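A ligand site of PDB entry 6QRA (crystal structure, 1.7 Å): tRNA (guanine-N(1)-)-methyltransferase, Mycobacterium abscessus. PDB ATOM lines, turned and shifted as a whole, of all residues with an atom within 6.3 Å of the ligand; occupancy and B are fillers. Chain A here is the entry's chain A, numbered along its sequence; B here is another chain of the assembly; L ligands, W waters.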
ATOM      1  N   PRO A  85     -19.431  23.802   4.712  1.00  0.00           N
ATOM      2  CA  PRO A  85     -20.672  23.056   4.974  1.00  0.00           C
ATOM      3  C   PRO A  85     -21.321  22.561   3.685  1.00  0.00           C
ATOM      4  O   PRO A  85     -21.322  23.264   2.667  1.00  0.00           O
ATOM      5  CB  PRO A  85     -21.561  24.093   5.653  1.00  0.00           C
ATOM      6  CG  PRO A  85     -20.606  25.067   6.312  1.00  0.00           C
ATOM      7  CD  PRO A  85     -19.462  25.156   5.290  1.00  0.00           C
ATOM      8  N   THR A  86     -21.893  21.350   3.735  1.00  0.00           N
ATOM      9  CA  THR A  86     -22.542  20.755   2.570  1.00  0.00           C
ATOM     10  C   THR A  86     -23.344  19.540   3.044  1.00  0.00           C
ATOM     11  O   THR A  86     -22.919  18.859   3.973  1.00  0.00           O
ATOM     12  CB  THR A  86     -21.530  20.334   1.469  1.00  0.00           C
ATOM     13  OG1 THR A  86     -22.158  19.423   0.548  1.00  0.00           O
ATOM     14  CG2 THR A  86     -20.302  19.670   2.089  1.00  0.00           C
ATOM     15  N   PRO A  87     -24.506  19.301   2.427  1.00  0.00           N
ATOM     16  CA  PRO A  87     -25.283  18.126   2.854  1.00  0.00           C
ATOM     17  C   PRO A  87     -24.598  16.830   2.442  1.00  0.00           C
ATOM     18  O   PRO A  87     -24.967  15.747   2.941  1.00  0.00           O
ATOM     19  CB  PRO A  87     -26.639  18.309   2.146  1.00  0.00           C
ATOM     20  CG  PRO A  87     -26.358  19.252   1.021  1.00  0.00           C
ATOM     21  CD  PRO A  87     -25.186  20.111   1.403  1.00  0.00           C
ATOM     22  N   ALA A  88     -23.589  16.931   1.589  1.00  0.00           N
ATOM     23  CA  ALA A  88     -22.821  15.755   1.168  1.00  0.00           C
ATOM     24  C   ALA A  88     -21.483  15.651   1.913  1.00  0.00           C
ATOM     25  O   ALA A  88     -20.596  14.954   1.477  1.00  0.00           O
ATOM     26  CB  ALA A  88     -22.572  15.786  -0.356  1.00  0.00           C
ATOM     27  N   ALA A 109     -16.598  28.630   4.521  1.00  0.00           N
ATOM     28  CA  ALA A 109     -17.149  29.039   3.222  1.00  0.00           C
ATOM     29  C   ALA A 109     -18.601  28.617   3.085  1.00  0.00           C
ATOM     30  O   ALA A 109     -18.886  27.420   2.905  1.00  0.00           O
ATOM     31  CB  ALA A 109     -16.316  28.438   2.111  1.00  0.00           C
ATOM     32  N   CYS A 110     -19.509  29.571   3.171  1.00  0.00           N
ATOM     33  CA  CYS A 110     -20.943  29.274   3.140  1.00  0.00           C
ATOM     34  C   CYS A 110     -21.509  29.352   1.736  1.00  0.00           C
ATOM     35  O   CYS A 110     -21.552  30.429   1.122  1.00  0.00           O
ATOM     36  CB  CYS A 110     -21.737  30.210   4.054  1.00  0.00           C
ATOM     37  SG  CYS A 110     -21.212  30.222   5.770  1.00  0.00           S
ATOM     38  N   GLY A 111     -21.958  28.216   1.243  1.00  0.00           N
ATOM     39  CA  GLY A 111     -22.572  28.153  -0.057  1.00  0.00           C
ATOM     40  C   GLY A 111     -24.035  28.531   0.004  1.00  0.00           C
ATOM     41  O   GLY A 111     -24.660  28.547   1.064  1.00  0.00           O
ATOM     42  N   ARG A 112     -24.568  28.841  -1.175  1.00  0.00           N
ATOM     43  CA  ARG A 112     -25.994  29.041  -1.371  1.00  0.00           C
ATOM     44  C   ARG A 112     -26.336  28.421  -2.710  1.00  0.00           C
ATOM     45  O   ARG A 112     -25.534  27.652  -3.262  1.00  0.00           O
ATOM     46  CB  ARG A 112     -26.368  30.522  -1.317  1.00  0.00           C
ATOM     47  CG  ARG A 112     -26.572  31.058   0.105  1.00  0.00           C
ATOM     48  CD  ARG A 112     -27.975  30.733   0.609  1.00  0.00           C
ATOM     49  NE  ARG A 112     -28.089  30.901   2.060  1.00  0.00           N
ATOM     50  CZ  ARG A 112     -29.244  30.949   2.709  1.00  0.00           C
ATOM     51  NH1 ARG A 112     -30.376  30.869   2.034  1.00  0.00           N
ATOM     52  NH2 ARG A 112     -29.268  31.100   4.027  1.00  0.00           N
ATOM     53  N   TYR A 113     -27.530  28.742  -3.241  1.00  0.00           N
ATOM     54  CA  TYR A 113     -27.990  28.129  -4.481  1.00  0.00           C
ATOM     55  C   TYR A 113     -27.911  26.623  -4.314  1.00  0.00           C
ATOM     56  O   TYR A 113     -28.397  26.103  -3.300  1.00  0.00           O
ATOM     57  CB  TYR A 113     -27.178  28.641  -5.686  1.00  0.00           C
ATOM     58  CG  TYR A 113     -27.180  30.160  -5.764  1.00  0.00           C
ATOM     59  CD1 TYR A 113     -28.171  30.836  -6.458  1.00  0.00           C
ATOM     60  CD2 TYR A 113     -26.217  30.911  -5.101  1.00  0.00           C
ATOM     61  CE1 TYR A 113     -28.189  32.220  -6.518  1.00  0.00           C
ATOM     62  CE2 TYR A 113     -26.232  32.298  -5.148  1.00  0.00           C
ATOM     63  CZ  TYR A 113     -27.219  32.946  -5.874  1.00  0.00           C
ATOM     64  OH  TYR A 113     -27.242  34.322  -5.930  1.00  0.00           O
ATOM     65  N   GLU A 114     -27.289  25.911  -5.242  1.00  0.00           N
ATOM     66  CA  GLU A 114     -27.181  24.463  -5.106  1.00  0.00           C
ATOM     67  C   GLU A 114     -25.765  23.983  -4.742  1.00  0.00           C
ATOM     68  O   GLU A 114     -25.440  22.804  -4.916  1.00  0.00           O
ATOM     69  CB  GLU A 114     -27.613  23.771  -6.393  1.00  0.00           C
ATOM     70  CG  GLU A 114     -28.995  24.162  -6.848  1.00  0.00           C
ATOM     71  CD  GLU A 114     -30.071  23.327  -6.220  1.00  0.00           C
ATOM     72  OE1 GLU A 114     -30.979  23.898  -5.579  1.00  0.00           O
ATOM     73  OE2 GLU A 114     -30.022  22.085  -6.372  1.00  0.00           O
ATOM     74  N   GLY A 115     -24.939  24.889  -4.228  1.00  0.00           N
ATOM     75  CA  GLY A 115     -23.612  24.511  -3.800  1.00  0.00           C
ATOM     76  C   GLY A 115     -22.518  25.215  -4.579  1.00  0.00           C
ATOM     77  O   GLY A 115     -22.808  26.066  -5.415  1.00  0.00           O
ATOM     78  N   ILE A 116     -21.270  24.852  -4.293  1.00  0.00           N
ATOM     79  CA  ILE A 116     -20.081  25.518  -4.846  1.00  0.00           C
ATOM     80  C   ILE A 116     -19.376  24.599  -5.824  1.00  0.00           C
ATOM     81  O   ILE A 116     -19.220  23.410  -5.550  1.00  0.00           O
ATOM     82  CB  ILE A 116     -19.105  25.916  -3.715  1.00  0.00           C
ATOM     83  CG1 ILE A 116     -19.840  26.721  -2.631  1.00  0.00           C
ATOM     84  CG2 ILE A 116     -17.898  26.683  -4.269  1.00  0.00           C
ATOM     85  CD1 ILE A 116     -18.984  26.987  -1.403  1.00  0.00           C
ATOM     86  N   VAL A 133     -18.124  19.318   5.396  1.00  0.00           N
ATOM     87  CA  VAL A 133     -18.839  18.684   6.502  1.00  0.00           C
ATOM     88  C   VAL A 133     -20.321  18.956   6.498  1.00  0.00           C
ATOM     89  O   VAL A 133     -20.788  19.992   6.045  1.00  0.00           O
ATOM     90  CB  VAL A 133     -18.299  19.122   7.903  1.00  0.00           C
ATOM     91  CG1 VAL A 133     -16.864  18.676   8.109  1.00  0.00           C
ATOM     92  CG2 VAL A 133     -18.431  20.660   8.105  1.00  0.00           C
ATOM     93  N   SER A 134     -21.059  17.974   7.015  1.00  0.00           N
ATOM     94  CA  SER A 134     -22.504  18.094   7.185  1.00  0.00           C
ATOM     95  C   SER A 134     -22.846  18.120   8.666  1.00  0.00           C
ATOM     96  O   SER A 134     -22.255  17.371   9.433  1.00  0.00           O
ATOM     97  CB  SER A 134     -23.203  16.917   6.512  1.00  0.00           C
ATOM     98  OG  SER A 134     -24.544  16.812   6.941  1.00  0.00           O
ATOM     99  N   ILE A 135     -23.814  18.954   9.057  1.00  0.00           N
ATOM    100  CA  ILE A 135     -24.196  19.016  10.471  1.00  0.00           C
ATOM    101  C   ILE A 135     -25.393  18.117  10.801  1.00  0.00           C
ATOM    102  O   ILE A 135     -25.816  18.053  11.957  1.00  0.00           O
ATOM    103  CB  ILE A 135     -24.518  20.454  10.915  1.00  0.00           C
ATOM    104  CG1 ILE A 135     -25.692  21.051  10.140  1.00  0.00           C
ATOM    105  CG2 ILE A 135     -23.252  21.349  10.825  1.00  0.00           C
ATOM    106  CD1 ILE A 135     -26.346  22.232  10.861  1.00  0.00           C
ATOM    107  N   GLY A 136     -25.913  17.417   9.796  1.00  0.00           N
ATOM    108  CA  GLY A 136     -27.026  16.512  10.037  1.00  0.00           C
ATOM    109  C   GLY A 136     -27.693  16.078   8.743  1.00  0.00           C
ATOM    110  O   GLY A 136     -27.456  16.668   7.685  1.00  0.00           O
ATOM    111  N   ASP A 137     -28.531  15.063   8.834  1.00  0.00           N
ATOM    112  CA  ASP A 137     -29.100  14.463   7.634  1.00  0.00           C
ATOM    113  C   ASP A 137     -30.394  15.136   7.195  1.00  0.00           C
ATOM    114  O   ASP A 137     -31.449  14.519   7.132  1.00  0.00           O
ATOM    115  CB  ASP A 137     -29.322  12.969   7.832  1.00  0.00           C
ATOM    116  CG  ASP A 137     -28.018  12.194   7.881  1.00  0.00           C
ATOM    117  OD1 ASP A 137     -27.021  12.678   7.298  1.00  0.00           O
ATOM    118  OD2 ASP A 137     -27.991  11.098   8.459  1.00  0.00           O
ATOM    119  N   TYR A 138     -30.268  16.421   6.873  1.00  0.00           N
ATOM    120  CA  TYR A 138     -31.374  17.243   6.389  1.00  0.00           C
ATOM    121  C   TYR A 138     -30.735  18.263   5.489  1.00  0.00           C
ATOM    122  O   TYR A 138     -29.519  18.458   5.537  1.00  0.00           O
ATOM    123  CB  TYR A 138     -32.153  17.903   7.539  1.00  0.00           C
ATOM    124  CG  TYR A 138     -31.239  18.390   8.632  1.00  0.00           C
ATOM    125  CD1 TYR A 138     -30.480  19.546   8.479  1.00  0.00           C
ATOM    126  CD2 TYR A 138     -31.064  17.647   9.795  1.00  0.00           C
ATOM    127  CE1 TYR A 138     -29.614  19.964   9.460  1.00  0.00           C
ATOM    128  CE2 TYR A 138     -30.195  18.069  10.789  1.00  0.00           C
ATOM    129  CZ  TYR A 138     -29.471  19.226  10.615  1.00  0.00           C
ATOM    130  OH  TYR A 138     -28.599  19.629  11.598  1.00  0.00           O
ATOM    131  N   VAL A 139     -31.546  18.891   4.638  1.00  0.00           N
ATOM    132  CA  VAL A 139     -31.043  19.882   3.698  1.00  0.00           C
ATOM    133  C   VAL A 139     -31.472  21.283   4.098  1.00  0.00           C
ATOM    134  O   VAL A 139     -32.657  21.548   4.296  1.00  0.00           O
ATOM    135  CB  VAL A 139     -31.529  19.586   2.267  1.00  0.00           C
ATOM    136  CG1 VAL A 139     -31.008  20.642   1.297  1.00  0.00           C
ATOM    137  CG2 VAL A 139     -31.089  18.191   1.840  1.00  0.00           C
ATOM    138  N   LEU A 140     -30.479  22.174   4.224  1.00  0.00           N
ATOM    139  CA  LEU A 140     -30.710  23.586   4.515  1.00  0.00           C
ATOM    140  C   LEU A 140     -30.779  24.359   3.203  1.00  0.00           C
ATOM    141  O   LEU A 140     -30.620  23.769   2.139  1.00  0.00           O
ATOM    142  CB  LEU A 140     -29.585  24.124   5.403  1.00  0.00           C
ATOM    143  CG  LEU A 140     -29.365  23.436   6.758  1.00  0.00           C
ATOM    144  CD1 LEU A 140     -28.000  23.788   7.300  1.00  0.00           C
ATOM    145  CD2 LEU A 140     -30.476  23.832   7.711  1.00  0.00           C
ATOM    146  N   ASN A 141     -30.997  25.666   3.277  1.00  0.00           N
ATOM    147  CA  ASN A 141     -30.993  26.506   2.079  1.00  0.00           C
ATOM    148  C   ASN A 141     -29.592  27.007   1.740  1.00  0.00           C
ATOM    149  O   ASN A 141     -29.346  27.493   0.632  1.00  0.00           O
ATOM    150  CB  ASN A 141     -31.918  27.707   2.262  1.00  0.00           C
ATOM    151  CG  ASN A 141     -33.374  27.366   2.014  1.00  0.00           C
ATOM    152  OD1 ASN A 141     -33.710  26.610   1.103  1.00  0.00           O
ATOM    153  ND2 ASN A 141     -34.257  27.943   2.820  1.00  0.00           N
ATOM    154  N   GLY A 142     -28.673  26.902   2.687  1.00  0.00           N
ATOM    155  CA  GLY A 142     -27.302  27.360   2.466  1.00  0.00           C
ATOM    156  C   GLY A 142     -26.459  27.032   3.666  1.00  0.00           C
ATOM    157  O   GLY A 142     -26.962  26.480   4.641  1.00  0.00           O
ATOM    158  N   GLY A 143     -25.181  27.410   3.642  1.00  0.00           N
ATOM    159  CA  GLY A 143     -24.278  27.009   4.709  1.00  0.00           C
ATOM    160  C   GLY A 143     -24.314  27.851   5.976  1.00  0.00           C
ATOM    161  O   GLY A 143     -23.652  27.499   6.966  1.00  0.00           O
ATOM    162  N   GLU A 144     -25.050  28.959   5.975  1.00  0.00           N
ATOM    163  CA  GLU A 144     -24.968  29.911   7.091  1.00  0.00           C
ATOM    164  C   GLU A 144     -25.480  29.321   8.402  1.00  0.00           C
ATOM    165  O   GLU A 144     -24.861  29.506   9.436  1.00  0.00           O
ATOM    166  CB  GLU A 144     -25.739  31.191   6.759  1.00  0.00           C
ATOM    167  CG  GLU A 144     -25.053  32.086   5.705  1.00  0.00           C
ATOM    168  CD  GLU A 144     -25.310  31.646   4.267  1.00  0.00           C
ATOM    169  OE1 GLU A 144     -26.149  30.742   4.027  1.00  0.00           O
ATOM    170  OE2 GLU A 144     -24.673  32.223   3.348  1.00  0.00           O
ATOM    171  N   ALA A 146     -25.468  26.234   9.211  1.00  0.00           N
ATOM    172  CA  ALA A 146     -24.433  25.276   9.568  1.00  0.00           C
ATOM    173  C   ALA A 146     -23.217  25.962  10.174  1.00  0.00           C
ATOM    174  O   ALA A 146     -22.614  25.447  11.109  1.00  0.00           O
ATOM    175  CB  ALA A 146     -24.021  24.447   8.349  1.00  0.00           C
ATOM    176  N   ARG B 156     -38.427  25.206   3.626  1.00  0.00           N
ATOM    177  CA  ARG B 156     -38.130  25.034   2.211  1.00  0.00           C
ATOM    178  C   ARG B 156     -38.939  23.881   1.599  1.00  0.00           C
ATOM    179  O   ARG B 156     -38.943  23.691   0.382  1.00  0.00           O
ATOM    180  CB  ARG B 156     -36.634  24.820   1.992  1.00  0.00           C
ATOM    181  CG  ARG B 156     -36.064  23.588   2.650  1.00  0.00           C
ATOM    182  CD  ARG B 156     -34.536  23.602   2.558  1.00  0.00           C
ATOM    183  NE  ARG B 156     -34.056  23.515   1.178  1.00  0.00           N
ATOM    184  CZ  ARG B 156     -34.065  22.402   0.448  1.00  0.00           C
ATOM    185  NH1 ARG B 156     -34.556  21.266   0.963  1.00  0.00           N
ATOM    186  NH2 ARG B 156     -33.617  22.413  -0.791  1.00  0.00           N
ATOM    187  N   ALA B 178     -31.575  11.227  -1.356  1.00  0.00           N
ATOM    188  CA  ALA B 178     -32.658  10.501  -0.695  1.00  0.00           C
ATOM    189  C   ALA B 178     -32.078   9.683   0.448  1.00  0.00           C
ATOM    190  O   ALA B 178     -32.266  10.011   1.627  1.00  0.00           O
ATOM    191  CB  ALA B 178     -33.380   9.623  -1.683  1.00  0.00           C
ATOM    192  N   LEU B 180     -28.737   8.960  -0.186  1.00  0.00           N
ATOM    193  CA  LEU B 180     -27.416   9.049  -0.825  1.00  0.00           C
ATOM    194  C   LEU B 180     -26.940  10.479  -0.757  1.00  0.00           C
ATOM    195  O   LEU B 180     -27.760  11.393  -0.744  1.00  0.00           O
ATOM    196  CB  LEU B 180     -27.488   8.605  -2.282  1.00  0.00           C
ATOM    197  CG  LEU B 180     -27.719   7.131  -2.600  1.00  0.00           C
ATOM    198  CD1 LEU B 180     -27.971   6.976  -4.085  1.00  0.00           C
ATOM    199  CD2 LEU B 180     -26.530   6.285  -2.162  1.00  0.00           C
ATOM    200  N   GLU B 182     -25.155  13.748  -2.491  1.00  0.00           N
ATOM    201  CA  GLU B 182     -25.044  14.313  -3.826  1.00  0.00           C
ATOM    202  C   GLU B 182     -23.595  14.362  -4.246  1.00  0.00           C
ATOM    203  O   GLU B 182     -22.733  14.606  -3.407  1.00  0.00           O
ATOM    204  CB  GLU B 182     -25.658  15.721  -3.863  1.00  0.00           C
ATOM    205  CG  GLU B 182     -26.725  15.921  -2.794  1.00  0.00           C
ATOM    206  CD  GLU B 182     -26.149  16.331  -1.462  1.00  0.00           C
ATOM    207  OE1 GLU B 182     -25.351  17.301  -1.425  1.00  0.00           O
ATOM    208  OE2 GLU B 182     -26.466  15.658  -0.452  1.00  0.00           O
HETATM  209  C1  LIG L   1     -24.323  24.379   2.239  1.00  0.00           C
HETATM  210  C2  LIG L   1     -26.478  25.366  -0.615  1.00  0.00           C
HETATM  211  C3  LIG L   1     -28.611  24.160  -0.280  1.00  0.00           C
HETATM  212  C4  LIG L   1     -27.627  22.043  -1.543  1.00  0.00           C
HETATM  213  C5  LIG L   1     -29.406  19.584  -3.908  1.00  0.00           C
HETATM  214  C6  LIG L   1     -29.421  17.434  -4.353  1.00  0.00           C
HETATM  215  C7  LIG L   1     -30.419  15.928  -2.661  1.00  0.00           C
HETATM  216  C8  LIG L   1     -30.219  18.325  -2.187  1.00  0.00           C
HETATM  217  C9  LIG L   1     -29.977  22.741  -1.754  1.00  0.00           C
HETATM  218  N1  LIG L   1     -25.959  19.414   6.853  1.00  0.00           N
HETATM  219  C10 LIG L   1     -26.359  20.327   5.819  1.00  0.00           C
HETATM  220  N2  LIG L   1     -27.640  20.435   5.314  1.00  0.00           N
HETATM  221  N3  LIG L   1     -27.650  21.417   4.331  1.00  0.00           N
HETATM  222  C11 LIG L   1     -26.425  21.937   4.231  1.00  0.00           C
HETATM  223  C12 LIG L   1     -26.015  22.938   3.230  1.00  0.00           C
HETATM  224  C13 LIG L   1     -26.935  23.198   2.196  1.00  0.00           C
HETATM  225  C14 LIG L   1     -26.528  24.088   1.172  1.00  0.00           C
HETATM  226  C15 LIG L   1     -25.268  24.667   1.198  1.00  0.00           C
HETATM  227  C16 LIG L   1     -24.706  23.487   3.265  1.00  0.00           C
HETATM  228  C17 LIG L   1     -25.215  25.472   0.056  1.00  0.00           C
HETATM  229  N4  LIG L   1     -27.222  24.543   0.050  1.00  0.00           N
HETATM  230  C18 LIG L   1     -28.752  22.944  -1.212  1.00  0.00           C
HETATM  231  C19 LIG L   1     -27.830  20.999  -2.383  1.00  0.00           C
HETATM  232  C20 LIG L   1     -29.139  20.766  -2.948  1.00  0.00           C
HETATM  233  N5  LIG L   1     -29.364  18.451  -3.362  1.00  0.00           N
HETATM  234  C21 LIG L   1     -30.275  16.189  -4.053  1.00  0.00           C
HETATM  235  C22 LIG L   1     -31.043  17.054  -2.047  1.00  0.00           C
HETATM  236  C23 LIG L   1     -30.192  21.636  -2.635  1.00  0.00           C
HETATM  237  C24 LIG L   1     -25.553  21.243   5.112  1.00  0.00           C
HETATM  238  O   HOH W   1     -23.731  22.328  -0.742  1.00  0.00           O
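O of Ile 135 is in hydrogen-bond range of OH of Tyr 138. The side-chain hydroxyl of Ser 134 sits at hydrogen-bond distance from the backbone carbonyl oxygen of Gly 136, 3.0 Å away. The backbone carbonyl oxygen (O) of Gly 111 is in hydrogen-bond range of the backbone NH (N) of Gly 143 (2.9 Å). The backbone NH (N) of Thr 86 is in hydrogen-bond range of the backbone carbonyl oxygen (O) of Val 133, at 2.9 Å. OG1 of Thr 86 sits close to N of Ala 88. OD1 of Asn 141 lies within hydrogen-bond range of NE of Arg 156 of chain B (3.1 Å). NE of Arg 112 lies within salt-bridge range of OE1 of Glu 144, 2.8 Å away.
The backbone NH of Ile 135 sits close to a nitrogen (N1) of the ligand (3.1 Å). Merely in contact with the ligand: Pro 85 (3.2 Å), Thr 86 (3.5 Å), Pro 87 (3.5 Å), Gly 111 (3.3 Å), Arg 112 (3.6 Å), Tyr 113 (3.4 Å), Glu 114 (3.6 Å), Gly 115 (3.96 Å), Val 139 (3.8 Å), Asn 141 (3.5 Å), Gly 142 (3.6 Å), Gly 143 (3.4 Å), Arg 156 of chain B (3.8 Å) and Glu 182 of chain B (3.5 Å). Hydrophobic or aromatic side chains within 4 Å of the ligand: Pro 85, Pro 87, Ile 135, Val 139 and Leu 140. Of the 29 residues printed, 19 come within 4 Å of the ligand.
A nitrogen (N2) of the ligand is in hydrogen-bond range of the backbone carbonyl oxygen of Tyr 138 (2.7 Å). N of Leu 140 lies within hydrogen-bond range of N3 of the ligand (2.9 Å). The side-chain hydroxyl (OG) of Ser 134 sits at hydrogen-bond distance from a nitrogen (N1) of the ligand, at 3.0 Å. A nitrogen (N1) of the ligand sits at hydrogen-bond distance from the backbone carbonyl oxygen of Gly 136 (3.2 Å).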
